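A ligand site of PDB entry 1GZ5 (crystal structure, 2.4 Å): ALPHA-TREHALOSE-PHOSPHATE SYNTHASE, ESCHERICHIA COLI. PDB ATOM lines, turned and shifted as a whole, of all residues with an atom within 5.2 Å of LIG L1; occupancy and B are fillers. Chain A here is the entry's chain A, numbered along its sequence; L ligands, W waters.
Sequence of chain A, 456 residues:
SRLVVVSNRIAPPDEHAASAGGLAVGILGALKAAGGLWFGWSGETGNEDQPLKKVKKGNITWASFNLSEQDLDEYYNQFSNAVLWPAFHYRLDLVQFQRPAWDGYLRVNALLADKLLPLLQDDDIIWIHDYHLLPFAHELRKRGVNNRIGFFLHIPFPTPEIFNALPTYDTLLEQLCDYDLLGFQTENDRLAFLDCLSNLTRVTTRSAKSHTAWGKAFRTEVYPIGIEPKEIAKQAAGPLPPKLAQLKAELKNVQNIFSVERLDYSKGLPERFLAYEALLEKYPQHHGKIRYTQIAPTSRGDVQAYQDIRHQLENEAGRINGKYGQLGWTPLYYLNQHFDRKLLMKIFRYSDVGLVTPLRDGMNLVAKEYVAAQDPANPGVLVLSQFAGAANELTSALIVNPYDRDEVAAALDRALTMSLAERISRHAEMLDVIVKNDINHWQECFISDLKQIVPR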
ATOM      1  N   ALA A  20     -17.198 -32.267 -21.645  1.00  0.00           N
ATOM      2  CA  ALA A  20     -17.613 -31.083 -20.913  1.00  0.00           C
ATOM      3  C   ALA A  20     -18.962 -30.688 -21.380  1.00  0.00           C
ATOM      4  O   ALA A  20     -19.272 -30.876 -22.543  1.00  0.00           O
ATOM      5  CB  ALA A  20     -16.658 -29.960 -21.169  1.00  0.00           C
ATOM      6  N   GLY A  21     -19.763 -30.149 -20.474  1.00  0.00           N
ATOM      7  CA  GLY A  21     -21.078 -29.654 -20.794  1.00  0.00           C
ATOM      8  C   GLY A  21     -22.107 -29.872 -19.697  1.00  0.00           C
ATOM      9  O   GLY A  21     -22.196 -30.957 -19.152  1.00  0.00           O
ATOM     10  N   GLY A  22     -22.897 -28.834 -19.380  1.00  0.00           N
ATOM     11  CA  GLY A  22     -23.725 -28.815 -18.202  1.00  0.00           C
ATOM     12  C   GLY A  22     -24.982 -29.639 -18.355  1.00  0.00           C
ATOM     13  O   GLY A  22     -25.500 -30.221 -17.349  1.00  0.00           O
ATOM     14  N   LEU A  23     -25.495 -29.688 -19.572  1.00  0.00           N
ATOM     15  CA  LEU A  23     -26.749 -30.411 -19.809  1.00  0.00           C
ATOM     16  C   LEU A  23     -26.671 -31.907 -19.321  1.00  0.00           C
ATOM     17  O   LEU A  23     -27.508 -32.413 -18.543  1.00  0.00           O
ATOM     18  CB  LEU A  23     -27.125 -30.351 -21.291  1.00  0.00           C
ATOM     19  CG  LEU A  23     -28.285 -31.257 -21.760  1.00  0.00           C
ATOM     20  CD1 LEU A  23     -29.064 -30.520 -22.811  1.00  0.00           C
ATOM     21  CD2 LEU A  23     -27.747 -32.614 -22.307  1.00  0.00           C
ATOM     22  N   VAL A  25     -24.563 -33.282 -17.368  1.00  0.00           N
ATOM     23  CA  VAL A  25     -24.372 -33.327 -15.911  1.00  0.00           C
ATOM     24  C   VAL A  25     -25.716 -33.175 -15.186  1.00  0.00           C
ATOM     25  O   VAL A  25     -26.038 -33.956 -14.254  1.00  0.00           O
ATOM     26  CB  VAL A  25     -23.367 -32.252 -15.430  1.00  0.00           C
ATOM     27  CG1 VAL A  25     -23.381 -32.112 -13.881  1.00  0.00           C
ATOM     28  CG2 VAL A  25     -21.938 -32.549 -15.943  1.00  0.00           C
ATOM     29  N   TRP A  85     -27.230 -21.853 -31.555  1.00  0.00           N
ATOM     30  CA  TRP A  85     -26.334 -21.483 -30.454  1.00  0.00           C
ATOM     31  C   TRP A  85     -25.887 -19.986 -30.540  1.00  0.00           C
ATOM     32  O   TRP A  85     -26.106 -19.245 -29.570  1.00  0.00           O
ATOM     33  CB  TRP A  85     -25.125 -22.399 -30.362  1.00  0.00           C
ATOM     34  CG  TRP A  85     -24.210 -21.978 -29.236  1.00  0.00           C
ATOM     35  CD1 TRP A  85     -23.173 -21.127 -29.291  1.00  0.00           C
ATOM     36  CD2 TRP A  85     -24.283 -22.423 -27.863  1.00  0.00           C
ATOM     37  NE1 TRP A  85     -22.594 -20.993 -28.067  1.00  0.00           N
ATOM     38  CE2 TRP A  85     -23.247 -21.784 -27.165  1.00  0.00           C
ATOM     39  CE3 TRP A  85     -25.128 -23.332 -27.162  1.00  0.00           C
ATOM     40  CZ2 TRP A  85     -23.002 -22.002 -25.780  1.00  0.00           C
ATOM     41  CZ3 TRP A  85     -24.892 -23.561 -25.801  1.00  0.00           C
ATOM     42  CH2 TRP A  85     -23.837 -22.911 -25.124  1.00  0.00           C
ATOM     43  N   VAL A 260     -12.871 -22.784 -15.466  1.00  0.00           N
ATOM     44  CA  VAL A 260     -12.984 -23.970 -16.330  1.00  0.00           C
ATOM     45  C   VAL A 260     -14.252 -23.863 -17.173  1.00  0.00           C
ATOM     46  O   VAL A 260     -15.300 -23.467 -16.650  1.00  0.00           O
ATOM     47  CB  VAL A 260     -12.804 -25.317 -15.571  1.00  0.00           C
ATOM     48  CG1 VAL A 260     -13.820 -25.483 -14.554  1.00  0.00           C
ATOM     49  CG2 VAL A 260     -12.958 -26.470 -16.502  1.00  0.00           C
ATOM     50  N   GLU A 261     -14.146 -24.120 -18.468  1.00  0.00           N
ATOM     51  CA  GLU A 261     -15.329 -24.186 -19.344  1.00  0.00           C
ATOM     52  C   GLU A 261     -14.932 -24.712 -20.690  1.00  0.00           C
ATOM     53  O   GLU A 261     -13.753 -24.686 -21.011  1.00  0.00           O
ATOM     54  CB  GLU A 261     -15.955 -22.843 -19.540  1.00  0.00           C
ATOM     55  CG  GLU A 261     -14.991 -21.674 -19.889  1.00  0.00           C
ATOM     56  CD  GLU A 261     -14.915 -20.695 -18.726  1.00  0.00           C
ATOM     57  OE1 GLU A 261     -15.799 -19.804 -18.617  1.00  0.00           O
ATOM     58  OE2 GLU A 261     -13.989 -20.852 -17.840  1.00  0.00           O
ATOM     59  N   ARG A 262     -15.894 -25.205 -21.446  1.00  0.00           N
ATOM     60  CA  ARG A 262     -15.710 -25.425 -22.881  1.00  0.00           C
ATOM     61  C   ARG A 262     -15.160 -24.166 -23.544  1.00  0.00           C
ATOM     62  O   ARG A 262     -15.526 -23.032 -23.215  1.00  0.00           O
ATOM     63  CB  ARG A 262     -17.045 -25.810 -23.542  1.00  0.00           C
ATOM     64  CG  ARG A 262     -17.618 -27.198 -23.158  1.00  0.00           C
ATOM     65  CD  ARG A 262     -19.030 -27.454 -23.835  1.00  0.00           C
ATOM     66  NE  ARG A 262     -19.924 -26.356 -23.564  1.00  0.00           N
ATOM     67  CZ  ARG A 262     -20.201 -25.360 -24.430  1.00  0.00           C
ATOM     68  NH1 ARG A 262     -19.726 -25.393 -25.679  1.00  0.00           N
ATOM     69  NH2 ARG A 262     -21.008 -24.350 -24.034  1.00  0.00           N
ATOM     70  N   LYS A 267     -18.439 -17.792 -23.574  1.00  0.00           N
ATOM     71  CA  LYS A 267     -17.764 -17.747 -22.269  1.00  0.00           C
ATOM     72  C   LYS A 267     -16.827 -16.555 -22.067  1.00  0.00           C
ATOM     73  O   LYS A 267     -16.325 -16.334 -20.938  1.00  0.00           O
ATOM     74  CB  LYS A 267     -16.982 -19.052 -22.044  1.00  0.00           C
ATOM     75  CG  LYS A 267     -17.803 -20.356 -22.221  1.00  0.00           C
ATOM     76  CD  LYS A 267     -18.797 -20.580 -21.067  1.00  0.00           C
ATOM     77  CE  LYS A 267     -19.615 -21.887 -21.309  1.00  0.00           C
ATOM     78  NZ  LYS A 267     -20.595 -22.152 -20.183  1.00  0.00           N
ATOM     79  N   ILE A 295      -8.809 -23.648 -17.697  1.00  0.00           N
ATOM     80  CA  ILE A 295      -8.958 -24.919 -18.381  1.00  0.00           C
ATOM     81  C   ILE A 295     -10.085 -24.789 -19.392  1.00  0.00           C
ATOM     82  O   ILE A 295     -11.176 -24.279 -19.057  1.00  0.00           O
ATOM     83  CB  ILE A 295      -9.232 -25.983 -17.397  1.00  0.00           C
ATOM     84  CG1 ILE A 295      -7.990 -26.131 -16.531  1.00  0.00           C
ATOM     85  CG2 ILE A 295      -9.604 -27.331 -18.121  1.00  0.00           C
ATOM     86  CD1 ILE A 295      -8.087 -27.313 -15.535  1.00  0.00           C
ATOM     87  N   PRO A 297     -11.212 -27.109 -22.608  1.00  0.00           N
ATOM     88  CA  PRO A 297     -11.211 -28.144 -23.633  1.00  0.00           C
ATOM     89  C   PRO A 297     -11.905 -27.632 -24.909  1.00  0.00           C
ATOM     90  O   PRO A 297     -12.885 -26.906 -24.840  1.00  0.00           O
ATOM     91  CB  PRO A 297     -12.043 -29.252 -22.973  1.00  0.00           C
ATOM     92  CG  PRO A 297     -12.904 -28.527 -22.034  1.00  0.00           C
ATOM     93  CD  PRO A 297     -12.025 -27.475 -21.441  1.00  0.00           C
ATOM     94  N   GLN A 337      -7.469 -28.549 -22.598  1.00  0.00           N
ATOM     95  CA  GLN A 337      -7.579 -29.990 -22.304  1.00  0.00           C
ATOM     96  C   GLN A 337      -8.843 -30.243 -21.489  1.00  0.00           C
ATOM     97  O   GLN A 337      -9.340 -29.353 -20.782  1.00  0.00           O
ATOM     98  CB  GLN A 337      -6.335 -30.482 -21.540  1.00  0.00           C
ATOM     99  CG  GLN A 337      -5.038 -30.145 -22.234  1.00  0.00           C
ATOM    100  CD  GLN A 337      -3.835 -30.354 -21.341  1.00  0.00           C
ATOM    101  OE1 GLN A 337      -3.839 -31.272 -20.525  1.00  0.00           O
ATOM    102  NE2 GLN A 337      -2.793 -29.511 -21.486  1.00  0.00           N
ATOM    103  N   HIS A 338      -9.365 -31.446 -21.608  1.00  0.00           N
ATOM    104  CA  HIS A 338     -10.491 -31.835 -20.823  1.00  0.00           C
ATOM    105  C   HIS A 338     -10.011 -32.442 -19.499  1.00  0.00           C
ATOM    106  O   HIS A 338      -9.103 -33.290 -19.480  1.00  0.00           O
ATOM    107  CB  HIS A 338     -11.322 -32.883 -21.595  1.00  0.00           C
ATOM    108  CG  HIS A 338     -12.339 -33.550 -20.735  1.00  0.00           C
ATOM    109  ND1 HIS A 338     -13.602 -33.030 -20.571  1.00  0.00           N
ATOM    110  CD2 HIS A 338     -12.259 -34.639 -19.920  1.00  0.00           C
ATOM    111  CE1 HIS A 338     -14.293 -33.808 -19.744  1.00  0.00           C
ATOM    112  NE2 HIS A 338     -13.495 -34.790 -19.332  1.00  0.00           N
ATOM    113  N   PHE A 339     -10.637 -32.036 -18.414  1.00  0.00           N
ATOM    114  CA  PHE A 339     -10.337 -32.622 -17.104  1.00  0.00           C
ATOM    115  C   PHE A 339     -11.582 -33.349 -16.558  1.00  0.00           C
ATOM    116  O   PHE A 339     -12.726 -32.895 -16.719  1.00  0.00           O
ATOM    117  CB  PHE A 339      -9.940 -31.534 -16.121  1.00  0.00           C
ATOM    118  CG  PHE A 339      -8.504 -31.109 -16.228  1.00  0.00           C
ATOM    119  CD1 PHE A 339      -8.046 -30.429 -17.350  1.00  0.00           C
ATOM    120  CD2 PHE A 339      -7.617 -31.406 -15.234  1.00  0.00           C
ATOM    121  CE1 PHE A 339      -6.710 -30.029 -17.447  1.00  0.00           C
ATOM    122  CE2 PHE A 339      -6.276 -31.030 -15.330  1.00  0.00           C
ATOM    123  CZ  PHE A 339      -5.824 -30.338 -16.446  1.00  0.00           C
ATOM    124  N   ASP A 340     -11.357 -34.495 -15.940  1.00  0.00           N
ATOM    125  CA  ASP A 340     -12.394 -35.256 -15.260  1.00  0.00           C
ATOM    126  C   ASP A 340     -13.079 -34.352 -14.235  1.00  0.00           C
ATOM    127  O   ASP A 340     -12.445 -33.578 -13.535  1.00  0.00           O
ATOM    128  CB  ASP A 340     -11.777 -36.531 -14.651  1.00  0.00           C
ATOM    129  CG  ASP A 340     -12.790 -37.410 -13.931  1.00  0.00           C
ATOM    130  OD1 ASP A 340     -14.016 -37.163 -14.000  1.00  0.00           O
ATOM    131  OD2 ASP A 340     -12.444 -38.426 -13.225  1.00  0.00           O
ATOM    132  N   ARG A 341     -14.398 -34.426 -14.186  1.00  0.00           N
ATOM    133  CA  ARG A 341     -15.216 -33.615 -13.288  1.00  0.00           C
ATOM    134  C   ARG A 341     -14.943 -33.901 -11.813  1.00  0.00           C
ATOM    135  O   ARG A 341     -14.929 -33.009 -10.992  1.00  0.00           O
ATOM    136  CB  ARG A 341     -16.693 -33.880 -13.601  1.00  0.00           C
ATOM    137  CG  ARG A 341     -17.613 -32.827 -13.072  1.00  0.00           C
ATOM    138  CD  ARG A 341     -19.052 -33.055 -13.476  1.00  0.00           C
ATOM    139  NE  ARG A 341     -19.893 -32.109 -12.752  1.00  0.00           N
ATOM    140  CZ  ARG A 341     -20.650 -32.414 -11.670  1.00  0.00           C
ATOM    141  NH1 ARG A 341     -20.683 -33.645 -11.176  1.00  0.00           N
ATOM    142  NH2 ARG A 341     -21.370 -31.450 -11.068  1.00  0.00           N
ATOM    143  N   LEU A 344     -11.962 -31.909 -11.016  1.00  0.00           N
ATOM    144  CA  LEU A 344     -12.218 -30.482 -10.990  1.00  0.00           C
ATOM    145  C   LEU A 344     -12.777 -30.044  -9.646  1.00  0.00           C
ATOM    146  O   LEU A 344     -12.463 -28.955  -9.165  1.00  0.00           O
ATOM    147  CB  LEU A 344     -13.172 -30.074 -12.138  1.00  0.00           C
ATOM    148  CG  LEU A 344     -12.588 -30.052 -13.548  1.00  0.00           C
ATOM    149  CD1 LEU A 344     -13.695 -29.824 -14.581  1.00  0.00           C
ATOM    150  CD2 LEU A 344     -11.536 -28.946 -13.634  1.00  0.00           C
ATOM    151  N   ASP A 361     -24.751 -16.778 -20.724  1.00  0.00           N
ATOM    152  CA  ASP A 361     -24.813 -18.177 -20.295  1.00  0.00           C
ATOM    153  C   ASP A 361     -26.172 -18.455 -19.730  1.00  0.00           C
ATOM    154  O   ASP A 361     -26.661 -17.720 -18.842  1.00  0.00           O
ATOM    155  CB  ASP A 361     -23.743 -18.366 -19.241  1.00  0.00           C
ATOM    156  CG  ASP A 361     -23.249 -19.805 -19.163  1.00  0.00           C
ATOM    157  OD1 ASP A 361     -24.143 -20.757 -19.040  1.00  0.00           O
ATOM    158  OD2 ASP A 361     -21.974 -20.054 -19.147  1.00  0.00           O
ATOM    159  N   ASN A 364     -24.858 -21.750 -15.970  1.00  0.00           N
ATOM    160  CA  ASN A 364     -23.481 -21.926 -15.645  1.00  0.00           C
ATOM    161  C   ASN A 364     -23.322 -22.786 -14.398  1.00  0.00           C
ATOM    162  O   ASN A 364     -23.350 -22.282 -13.287  1.00  0.00           O
ATOM    163  CB  ASN A 364     -22.680 -20.630 -15.533  1.00  0.00           C
ATOM    164  CG  ASN A 364     -21.181 -20.905 -15.534  1.00  0.00           C
ATOM    165  OD1 ASN A 364     -20.645 -21.474 -14.551  1.00  0.00           O
ATOM    166  ND2 ASN A 364     -20.511 -20.618 -16.639  1.00  0.00           N
ATOM    167  N   LEU A 365     -23.141 -24.099 -14.574  1.00  0.00           N
ATOM    168  CA  LEU A 365     -23.012 -24.989 -13.450  1.00  0.00           C
ATOM    169  C   LEU A 365     -21.641 -24.895 -12.812  1.00  0.00           C
ATOM    170  O   LEU A 365     -21.497 -25.128 -11.629  1.00  0.00           O
ATOM    171  CB  LEU A 365     -23.329 -26.464 -13.809  1.00  0.00           C
ATOM    172  CG  LEU A 365     -24.789 -26.742 -14.206  1.00  0.00           C
ATOM    173  CD1 LEU A 365     -24.989 -28.214 -14.413  1.00  0.00           C
ATOM    174  CD2 LEU A 365     -25.751 -26.174 -13.175  1.00  0.00           C
ATOM    175  N   VAL A 366     -20.632 -24.528 -13.573  1.00  0.00           N
ATOM    176  CA  VAL A 366     -19.299 -24.391 -12.999  1.00  0.00           C
ATOM    177  C   VAL A 366     -19.348 -23.463 -11.778  1.00  0.00           C
ATOM    178  O   VAL A 366     -18.745 -23.770 -10.758  1.00  0.00           O
ATOM    179  CB  VAL A 366     -18.295 -23.934 -14.061  1.00  0.00           C
ATOM    180  CG1 VAL A 366     -17.040 -23.311 -13.409  1.00  0.00           C
ATOM    181  CG2 VAL A 366     -17.882 -25.127 -14.872  1.00  0.00           C
ATOM    182  N   GLU A 369     -20.867 -25.374  -8.912  1.00  0.00           N
ATOM    183  CA  GLU A 369     -19.922 -26.436  -8.512  1.00  0.00           C
ATOM    184  C   GLU A 369     -18.802 -25.834  -7.671  1.00  0.00           C
ATOM    185  O   GLU A 369     -18.363 -26.432  -6.703  1.00  0.00           O
ATOM    186  CB  GLU A 369     -19.330 -27.161  -9.738  1.00  0.00           C
ATOM    187  CG  GLU A 369     -20.330 -28.092 -10.417  1.00  0.00           C
ATOM    188  CD  GLU A 369     -19.968 -28.508 -11.835  1.00  0.00           C
ATOM    189  OE1 GLU A 369     -20.691 -29.403 -12.357  1.00  0.00           O
ATOM    190  OE2 GLU A 369     -18.993 -27.991 -12.472  1.00  0.00           O
HETATM  191  N1  LIG L   1     -16.624 -29.698 -17.196  1.00  0.00           N
HETATM  192  C1  LIG L   1     -15.883 -30.864 -17.098  1.00  0.00           C
HETATM  193  N2  LIG L   1     -14.570 -30.949 -17.569  1.00  0.00           N
HETATM  194  C2  LIG L   1     -14.021 -29.837 -18.176  1.00  0.00           C
HETATM  195  C3  LIG L   1     -14.791 -28.660 -18.351  1.00  0.00           C
HETATM  196  C4  LIG L   1     -16.112 -28.606 -17.880  1.00  0.00           C
HETATM  197  O1  LIG L   1     -16.427 -31.819 -16.544  1.00  0.00           O
HETATM  198  O2  LIG L   1     -12.865 -29.943 -18.615  1.00  0.00           O
HETATM  199  C5  LIG L   1     -17.966 -29.797 -16.700  1.00  0.00           C
HETATM  200  C6  LIG L   1     -18.146 -28.804 -15.626  1.00  0.00           C
HETATM  201  O3  LIG L   1     -17.683 -29.346 -14.427  1.00  0.00           O
HETATM  202  C7  LIG L   1     -19.634 -28.577 -15.698  1.00  0.00           C
HETATM  203  C8  LIG L   1     -19.928 -28.667 -17.173  1.00  0.00           C
HETATM  204  O4  LIG L   1     -18.822 -29.379 -17.732  1.00  0.00           O
HETATM  205  O5  LIG L   1     -20.387 -29.550 -14.993  1.00  0.00           O
HETATM  206  C9  LIG L   1     -19.971 -27.235 -17.743  1.00  0.00           C
HETATM  207  O6  LIG L   1     -21.312 -26.852 -17.657  1.00  0.00           O
HETATM  208  P1  LIG L   1     -21.625 -25.291 -17.616  1.00  0.00           P
HETATM  209  O7  LIG L   1     -23.012 -25.067 -17.234  1.00  0.00           O
HETATM  210  O8  LIG L   1     -20.667 -24.463 -16.837  1.00  0.00           O
HETATM  211  O9  LIG L   1     -21.273 -24.791 -19.116  1.00  0.00           O
HETATM  212  P2  LIG L   1     -21.752 -25.392 -20.471  1.00  0.00           P
HETATM  213  O10 LIG L   1     -22.934 -26.272 -20.335  1.00  0.00           O
HETATM  214  O11 LIG L   1     -20.691 -26.256 -21.055  1.00  0.00           O
HETATM  215  O12 LIG L   1     -21.895 -24.212 -21.371  1.00  0.00           O
HETATM  216  C1  LG2 L   2     -24.353 -26.861 -23.476  1.00  0.00           C
HETATM  217  C2  LG2 L   2     -25.639 -27.186 -24.211  1.00  0.00           C
HETATM  218  C3  LG2 L   2     -25.862 -28.707 -24.259  1.00  0.00           C
HETATM  219  C4  LG2 L   2     -24.585 -29.304 -24.809  1.00  0.00           C
HETATM  220  C5  LG2 L   2     -23.389 -28.934 -23.977  1.00  0.00           C
HETATM  221  C6  LG2 L   2     -22.123 -29.463 -24.597  1.00  0.00           C
HETATM  222  O1  LG2 L   2     -24.429 -27.270 -22.187  1.00  0.00           O
HETATM  223  O2  LG2 L   2     -26.647 -26.511 -23.488  1.00  0.00           O
HETATM  224  O3  LG2 L   2     -26.938 -29.016 -25.177  1.00  0.00           O
HETATM  225  O4  LG2 L   2     -24.656 -30.704 -24.885  1.00  0.00           O
HETATM  226  O5  LG2 L   2     -23.251 -27.505 -24.075  1.00  0.00           O
HETATM  227  O6  LG2 L   2     -22.071 -29.303 -26.013  1.00  0.00           O
HETATM  228  P1  LG2 L   2     -22.017 -30.511 -27.109  1.00  0.00           P
HETATM  229  O7  LG2 L   2     -20.643 -31.061 -27.110  1.00  0.00           O
HETATM  230  O8  LG2 L   2     -22.268 -29.764 -28.349  1.00  0.00           O
HETATM  231  O9  LG2 L   2     -23.157 -31.387 -26.624  1.00  0.00           O
HETATM  232  O   HOH W   1     -18.682 -25.089 -20.065  1.00  0.00           O
HETATM  233  O   HOH W   2     -25.174 -23.057 -18.532  1.00  0.00           O
HETATM  234  O   HOH W   3     -18.999 -23.117 -18.144  1.00  0.00           O
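N of Val 366 is in hydrogen-bond range of O8 of LIG L1, at 3.3 Å.
O7 of LIG L1 sits at hydrogen-bond distance from N of Leu 365, at 2.8 Å.
An oxygen (O5) of LIG L1 sits at hydrogen-bond distance from the side-chain carboxylate (OE1) of Glu 369 (2.7 Å).
The backbone NH (N) of Gly 21 sits at hydrogen-bond distance from an oxygen (O4) of LIG L1, 3.0 Å away.
The side-chain amino group of Lys 267 is in salt-bridge range of an oxygen (O12) of LIG L1 (2.7 Å).
O11 of LIG L1 is in salt-bridge range of NE of Arg 262, 2.6 Å away.
NE of Arg 341 is in hydrogen-bond range of O5 of LIG L1 (3.4 Å).
The backbone NH (N) of Phe 339 lies within hydrogen-bond range of an oxygen (O2) of LIG L1.
N of Gly 22 is in hydrogen-bond range of O10 of LIG L1.
The backbone carbonyl oxygen of Phe 339 sits at hydrogen-bond distance from a nitrogen (N2) of LIG L1, at 2.8 Å.
An oxygen (O10) of LIG L1 lies within hydrogen-bond range of an oxygen (O1) of LG2 L2.
OE1 of Glu 369 is in salt-bridge range of NH2 of Arg 341.
The side-chain carboxylate (OD2) of Asp 361 is in salt-bridge range of the side-chain amino group (NZ) of Lys 267.
The side-chain amide nitrogen (ND2) of Asn 364 lies within hydrogen-bond range of the side-chain carboxylate (OD2) of Asp 361 (3.0 Å).
The side-chain amide oxygen (OD1) of Asn 364 sits at hydrogen-bond distance from the backbone NH (N) of Val 366 (3.2 Å).
Merely in contact with LIG L1: Leu 344, Val 260, Val 25, Asn 364, Ala 20, His 338 and Pro 297.
Hydrophobic or aromatic side chains within 4 Å of LIG L1: Ala 20, Val 25, Val 260, Pro 297, His 338, Leu 344, Leu 365 and Val 366.
Within 4 Å of LIG L1: Ala 20, Gly 21, Gly 22, Val 25, Val 260, Arg 262, Lys 267, Pro 297, His 338, Phe 339, Arg 341, Leu 344, Asn 364, Leu 365, Val 366 and Glu 369.
Water W3 lies within hydrogen-bond range of O8 of LIG L1 (2.5 Å), NZ of Lys 267 (2.8 Å) and ND2 of Asn 364 (3.3 Å).
Water W1 bridges O11 of LIG L1 (2.5 Å) and N of Arg 262 (3.1 Å).
Water W2 lies within hydrogen-bond range of OD1 of Asp 361, N of Asn 364 and O7 of LIG L1.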
